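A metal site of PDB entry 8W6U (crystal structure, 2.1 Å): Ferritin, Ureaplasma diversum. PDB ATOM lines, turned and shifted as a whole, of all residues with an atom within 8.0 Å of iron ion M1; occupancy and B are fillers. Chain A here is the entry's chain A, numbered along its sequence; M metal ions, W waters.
Of the 19 residues printed, 4 come within 4 Å of iron ion M1.
The side-chain carboxylate of Asp 138 lies within salt-bridge range of the guanidinium group of Arg 137, at 3.1 Å.
NZ of Lys 61 sits close to OD2 of Asp 142, 3.1 Å away.
A ring nitrogen (ND1) of His 65 is in hydrogen-bond range of the side-chain amide oxygen (OD1) of Asn 27, at 3.3 Å.
O of His 65 sits at hydrogen-bond distance from OH of Tyr 135 (2.8 Å).
Water W1 lies within hydrogen-bond range of OD1 of Asp 60 and OD1 of Asp 138.
Iron ion M1 is bound by OD2 of Asp 60 (2.0 Å), water W1 (2.1 Å), OD2 of Asp 138 (2.1 Å), OD2 of Asp 142 (2.1 Å) and NE2 of His 65 (2.2 Å).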
ATOM      1  N   ASN A  27     -32.156  -8.420  -0.401  1.00  0.00           N
ATOM      2  CA  ASN A  27     -30.996  -7.690  -0.904  1.00  0.00           C
ATOM      3  C   ASN A  27     -31.407  -6.394  -1.606  1.00  0.00           C
ATOM      4  O   ASN A  27     -30.701  -5.377  -1.494  1.00  0.00           O
ATOM      5  CB  ASN A  27     -30.191  -8.589  -1.832  1.00  0.00           C
ATOM      6  CG  ASN A  27     -29.210  -9.436  -1.068  1.00  0.00           C
ATOM      7  OD1 ASN A  27     -28.209  -8.931  -0.593  1.00  0.00           O
ATOM      8  ND2 ASN A  27     -29.522 -10.722  -0.897  1.00  0.00           N
ATOM      9  N   HIS A  56     -21.058   1.758  -1.110  1.00  0.00           N
ATOM     10  CA  HIS A  56     -20.442   0.625  -1.763  1.00  0.00           C
ATOM     11  C   HIS A  56     -21.217  -0.616  -1.374  1.00  0.00           C
ATOM     12  O   HIS A  56     -21.487  -1.446  -2.191  1.00  0.00           O
ATOM     13  CB  HIS A  56     -18.962   0.573  -1.406  1.00  0.00           C
ATOM     14  CG  HIS A  56     -18.236  -0.605  -1.979  1.00  0.00           C
ATOM     15  ND1 HIS A  56     -17.618  -0.571  -3.215  1.00  0.00           N
ATOM     16  CD2 HIS A  56     -18.018  -1.845  -1.485  1.00  0.00           C
ATOM     17  CE1 HIS A  56     -17.058  -1.742  -3.457  1.00  0.00           C
ATOM     18  NE2 HIS A  56     -17.280  -2.533  -2.420  1.00  0.00           N
ATOM     19  N   LEU A  57     -21.591  -0.701  -0.122  1.00  0.00           N
ATOM     20  CA  LEU A  57     -22.409  -1.801   0.323  1.00  0.00           C
ATOM     21  C   LEU A  57     -23.794  -1.811  -0.324  1.00  0.00           C
ATOM     22  O   LEU A  57     -24.259  -2.851  -0.674  1.00  0.00           O
ATOM     23  CB  LEU A  57     -22.439  -1.832   1.850  1.00  0.00           C
ATOM     24  CG  LEU A  57     -22.828  -3.123   2.561  1.00  0.00           C
ATOM     25  CD1 LEU A  57     -21.971  -4.291   2.119  1.00  0.00           C
ATOM     26  CD2 LEU A  57     -22.729  -2.911   4.054  1.00  0.00           C
ATOM     27  N   GLU A  59     -24.553  -0.784  -3.279  1.00  0.00           N
ATOM     28  CA  GLU A  59     -24.328  -1.268  -4.607  1.00  0.00           C
ATOM     29  C   GLU A  59     -23.971  -2.758  -4.681  1.00  0.00           C
ATOM     30  O   GLU A  59     -24.261  -3.393  -5.638  1.00  0.00           O
ATOM     31  CB  GLU A  59     -23.312  -0.395  -5.288  1.00  0.00           C
ATOM     32  CG  GLU A  59     -23.784   1.031  -5.503  1.00  0.00           C
ATOM     33  CD  GLU A  59     -22.648   1.993  -5.799  1.00  0.00           C
ATOM     34  OE1 GLU A  59     -22.880   3.206  -5.755  1.00  0.00           O
ATOM     35  OE2 GLU A  59     -21.538   1.540  -6.093  1.00  0.00           O
ATOM     36  N   ASP A  60     -23.354  -3.299  -3.661  1.00  0.00           N
ATOM     37  CA  ASP A  60     -23.088  -4.717  -3.602  1.00  0.00           C
ATOM     38  C   ASP A  60     -24.422  -5.464  -3.525  1.00  0.00           C
ATOM     39  O   ASP A  60     -24.653  -6.356  -4.298  1.00  0.00           O
ATOM     40  CB  ASP A  60     -22.218  -4.990  -2.380  1.00  0.00           C
ATOM     41  CG  ASP A  60     -21.773  -6.395  -2.272  1.00  0.00           C
ATOM     42  OD1 ASP A  60     -21.426  -6.983  -3.297  1.00  0.00           O
ATOM     43  OD2 ASP A  60     -21.753  -6.915  -1.139  1.00  0.00           O
ATOM     44  N   LYS A  61     -25.298  -5.048  -2.631  1.00  0.00           N
ATOM     45  CA  LYS A  61     -26.586  -5.704  -2.448  1.00  0.00           C
ATOM     46  C   LYS A  61     -27.473  -5.626  -3.658  1.00  0.00           C
ATOM     47  O   LYS A  61     -28.077  -6.602  -4.051  1.00  0.00           O
ATOM     48  CB  LYS A  61     -27.311  -5.138  -1.228  1.00  0.00           C
ATOM     49  CG  LYS A  61     -26.551  -5.125   0.071  1.00  0.00           C
ATOM     50  CD  LYS A  61     -26.027  -6.496   0.438  1.00  0.00           C
ATOM     51  CE  LYS A  61     -25.398  -6.462   1.811  1.00  0.00           C
ATOM     52  NZ  LYS A  61     -24.651  -7.693   2.134  1.00  0.00           N
ATOM     53  N   VAL A  64     -24.437  -7.573  -7.501  1.00  0.00           N
ATOM     54  CA  VAL A  64     -24.199  -8.994  -7.554  1.00  0.00           C
ATOM     55  C   VAL A  64     -25.060  -9.894  -6.678  1.00  0.00           C
ATOM     56  O   VAL A  64     -25.440 -10.952  -7.100  1.00  0.00           O
ATOM     57  CB  VAL A  64     -22.701  -9.323  -7.405  1.00  0.00           C
ATOM     58  CG1 VAL A  64     -21.915  -8.797  -8.580  1.00  0.00           C
ATOM     59  CG2 VAL A  64     -22.134  -8.807  -6.099  1.00  0.00           C
ATOM     60  N   HIS A  65     -25.369  -9.454  -5.485  1.00  0.00           N
ATOM     61  CA  HIS A  65     -26.188 -10.224  -4.604  1.00  0.00           C
ATOM     62  C   HIS A  65     -27.526 -10.587  -5.236  1.00  0.00           C
ATOM     63  O   HIS A  65     -27.983 -11.692  -5.108  1.00  0.00           O
ATOM     64  CB  HIS A  65     -26.408  -9.489  -3.307  1.00  0.00           C
ATOM     65  CG  HIS A  65     -25.265  -9.560  -2.349  1.00  0.00           C
ATOM     66  ND1 HIS A  65     -25.300 -10.317  -1.209  1.00  0.00           N
ATOM     67  CD2 HIS A  65     -24.067  -8.920  -2.342  1.00  0.00           C
ATOM     68  CE1 HIS A  65     -24.164 -10.170  -0.548  1.00  0.00           C
ATOM     69  NE2 HIS A  65     -23.407  -9.327  -1.217  1.00  0.00           N
ATOM     70  N   GLU A 106     -26.503  -7.107   8.686  1.00  0.00           N
ATOM     71  CA  GLU A 106     -25.602  -8.092   8.091  1.00  0.00           C
ATOM     72  C   GLU A 106     -25.586  -9.387   8.883  1.00  0.00           C
ATOM     73  O   GLU A 106     -25.450 -10.436   8.329  1.00  0.00           O
ATOM     74  CB  GLU A 106     -24.212  -7.487   7.919  1.00  0.00           C
ATOM     75  CG  GLU A 106     -24.141  -6.295   7.001  1.00  0.00           C
ATOM     76  CD  GLU A 106     -24.543  -6.633   5.582  1.00  0.00           C
ATOM     77  OE1 GLU A 106     -23.861  -7.452   4.950  1.00  0.00           O
ATOM     78  OE2 GLU A 106     -25.512  -6.078   5.081  1.00  0.00           O
ATOM     79  N   VAL A 109     -28.413 -11.322   7.759  1.00  0.00           N
ATOM     80  CA  VAL A 109     -28.131 -11.920   6.473  1.00  0.00           C
ATOM     81  C   VAL A 109     -27.531 -13.282   6.669  1.00  0.00           C
ATOM     82  O   VAL A 109     -27.974 -14.226   6.089  1.00  0.00           O
ATOM     83  CB  VAL A 109     -27.233 -11.009   5.576  1.00  0.00           C
ATOM     84  CG1 VAL A 109     -26.655 -11.767   4.392  1.00  0.00           C
ATOM     85  CG2 VAL A 109     -28.002  -9.794   5.104  1.00  0.00           C
ATOM     86  N   TRP A 134     -21.382 -19.077  -2.004  1.00  0.00           N
ATOM     87  CA  TRP A 134     -20.953 -17.705  -2.216  1.00  0.00           C
ATOM     88  C   TRP A 134     -21.565 -16.816  -1.159  1.00  0.00           C
ATOM     89  O   TRP A 134     -20.872 -16.040  -0.563  1.00  0.00           O
ATOM     90  CB  TRP A 134     -21.339 -17.243  -3.621  1.00  0.00           C
ATOM     91  CG  TRP A 134     -20.835 -15.886  -4.010  1.00  0.00           C
ATOM     92  CD1 TRP A 134     -19.709 -15.617  -4.716  1.00  0.00           C
ATOM     93  CD2 TRP A 134     -21.455 -14.615  -3.753  1.00  0.00           C
ATOM     94  NE1 TRP A 134     -19.578 -14.268  -4.902  1.00  0.00           N
ATOM     95  CE2 TRP A 134     -20.638 -13.632  -4.312  1.00  0.00           C
ATOM     96  CE3 TRP A 134     -22.610 -14.224  -3.093  1.00  0.00           C
ATOM     97  CZ2 TRP A 134     -20.929 -12.277  -4.230  1.00  0.00           C
ATOM     98  CZ3 TRP A 134     -22.905 -12.884  -3.019  1.00  0.00           C
ATOM     99  CH2 TRP A 134     -22.078 -11.931  -3.577  1.00  0.00           C
ATOM    100  N   TYR A 135     -22.850 -16.967  -0.932  1.00  0.00           N
ATOM    101  CA  TYR A 135     -23.558 -16.188   0.058  1.00  0.00           C
ATOM    102  C   TYR A 135     -23.164 -16.507   1.495  1.00  0.00           C
ATOM    103  O   TYR A 135     -23.137 -15.643   2.312  1.00  0.00           O
ATOM    104  CB  TYR A 135     -25.044 -16.333  -0.181  1.00  0.00           C
ATOM    105  CG  TYR A 135     -25.519 -15.760  -1.497  1.00  0.00           C
ATOM    106  CD1 TYR A 135     -25.429 -16.489  -2.671  1.00  0.00           C
ATOM    107  CD2 TYR A 135     -26.064 -14.492  -1.566  1.00  0.00           C
ATOM    108  CE1 TYR A 135     -25.853 -15.959  -3.865  1.00  0.00           C
ATOM    109  CE2 TYR A 135     -26.491 -13.959  -2.750  1.00  0.00           C
ATOM    110  CZ  TYR A 135     -26.383 -14.698  -3.903  1.00  0.00           C
ATOM    111  OH  TYR A 135     -26.816 -14.186  -5.083  1.00  0.00           O
ATOM    112  N   ARG A 137     -20.132 -17.432   2.416  1.00  0.00           N
ATOM    113  CA  ARG A 137     -18.853 -16.778   2.565  1.00  0.00           C
ATOM    114  C   ARG A 137     -19.012 -15.286   2.676  1.00  0.00           C
ATOM    115  O   ARG A 137     -18.439 -14.663   3.520  1.00  0.00           O
ATOM    116  CB  ARG A 137     -17.964 -17.159   1.398  1.00  0.00           C
ATOM    117  CG  ARG A 137     -16.645 -16.421   1.306  1.00  0.00           C
ATOM    118  CD  ARG A 137     -16.178 -16.256  -0.141  1.00  0.00           C
ATOM    119  NE  ARG A 137     -17.180 -15.685  -1.029  1.00  0.00           N
ATOM    120  CZ  ARG A 137     -17.493 -14.395  -1.084  1.00  0.00           C
ATOM    121  NH1 ARG A 137     -16.910 -13.502  -0.309  1.00  0.00           N
ATOM    122  NH2 ARG A 137     -18.425 -13.987  -1.922  1.00  0.00           N
ATOM    123  N   ASP A 138     -19.839 -14.735   1.811  1.00  0.00           N
ATOM    124  CA  ASP A 138     -20.056 -13.319   1.806  1.00  0.00           C
ATOM    125  C   ASP A 138     -20.749 -12.780   3.024  1.00  0.00           C
ATOM    126  O   ASP A 138     -20.505 -11.661   3.395  1.00  0.00           O
ATOM    127  CB  ASP A 138     -20.771 -12.924   0.561  1.00  0.00           C
ATOM    128  CG  ASP A 138     -20.374 -11.582   0.075  1.00  0.00           C
ATOM    129  OD1 ASP A 138     -19.248 -11.444  -0.395  1.00  0.00           O
ATOM    130  OD2 ASP A 138     -21.180 -10.665   0.181  1.00  0.00           O
ATOM    131  N   GLY A 139     -21.594 -13.573   3.643  1.00  0.00           N
ATOM    132  CA  GLY A 139     -22.202 -13.188   4.893  1.00  0.00           C
ATOM    133  C   GLY A 139     -21.181 -12.738   5.894  1.00  0.00           C
ATOM    134  O   GLY A 139     -21.280 -11.677   6.460  1.00  0.00           O
ATOM    135  N   LYS A 141     -17.821 -12.114   5.260  1.00  0.00           N
ATOM    136  CA  LYS A 141     -16.972 -11.083   4.725  1.00  0.00           C
ATOM    137  C   LYS A 141     -17.555  -9.714   4.870  1.00  0.00           C
ATOM    138  O   LYS A 141     -16.907  -8.817   5.347  1.00  0.00           O
ATOM    139  CB  LYS A 141     -16.653 -11.372   3.282  1.00  0.00           C
ATOM    140  CG  LYS A 141     -15.735 -10.377   2.606  1.00  0.00           C
ATOM    141  CD  LYS A 141     -16.342  -9.940   1.293  1.00  0.00           C
ATOM    142  CE  LYS A 141     -15.272  -9.498   0.316  1.00  0.00           C
ATOM    143  NZ  LYS A 141     -15.863  -9.135  -1.003  1.00  0.00           N
ATOM    144  N   ASP A 142     -18.800  -9.577   4.488  1.00  0.00           N
ATOM    145  CA  ASP A 142     -19.463  -8.301   4.603  1.00  0.00           C
ATOM    146  C   ASP A 142     -19.613  -7.865   6.054  1.00  0.00           C
ATOM    147  O   ASP A 142     -19.426  -6.723   6.372  1.00  0.00           O
ATOM    148  CB  ASP A 142     -20.785  -8.318   3.839  1.00  0.00           C
ATOM    149  CG  ASP A 142     -20.623  -8.118   2.343  1.00  0.00           C
ATOM    150  OD1 ASP A 142     -19.508  -7.860   1.882  1.00  0.00           O
ATOM    151  OD2 ASP A 142     -21.624  -8.213   1.624  1.00  0.00           O
ATOM    152  N   LEU A 143     -19.910  -8.788   6.949  1.00  0.00           N
ATOM    153  CA  LEU A 143     -19.995  -8.471   8.360  1.00  0.00           C
ATOM    154  C   LEU A 143     -18.673  -8.003   8.901  1.00  0.00           C
ATOM    155  O   LEU A 143     -18.638  -7.103   9.690  1.00  0.00           O
ATOM    156  CB  LEU A 143     -20.475  -9.659   9.172  1.00  0.00           C
ATOM    157  CG  LEU A 143     -20.766  -9.410  10.637  1.00  0.00           C
ATOM    158  CD1 LEU A 143     -22.195  -8.948  10.817  1.00  0.00           C
ATOM    159  CD2 LEU A 143     -20.463 -10.624  11.483  1.00  0.00           C
ATOM    160  N   GLU A 145     -16.228  -6.494   7.264  1.00  0.00           N
ATOM    161  CA  GLU A 145     -15.957  -5.153   6.792  1.00  0.00           C
ATOM    162  C   GLU A 145     -16.738  -4.125   7.583  1.00  0.00           C
ATOM    163  O   GLU A 145     -16.213  -3.096   7.929  1.00  0.00           O
ATOM    164  CB  GLU A 145     -16.189  -5.060   5.294  1.00  0.00           C
ATOM    165  CG  GLU A 145     -15.306  -5.976   4.482  1.00  0.00           C
ATOM    166  CD  GLU A 145     -15.554  -5.898   2.981  1.00  0.00           C
ATOM    167  OE1 GLU A 145     -16.573  -5.313   2.563  1.00  0.00           O
ATOM    168  OE2 GLU A 145     -14.720  -6.432   2.235  1.00  0.00           O
HETATM  169 FE    FE M   1     -21.454  -8.710  -0.429  1.00  0.00          FE
HETATM  170 FE    FE M   2     -16.743  -4.896  -1.624  1.00  0.00          FE
HETATM  171  O   HOH W   1     -20.167  -9.201  -1.957  1.00  0.00           O
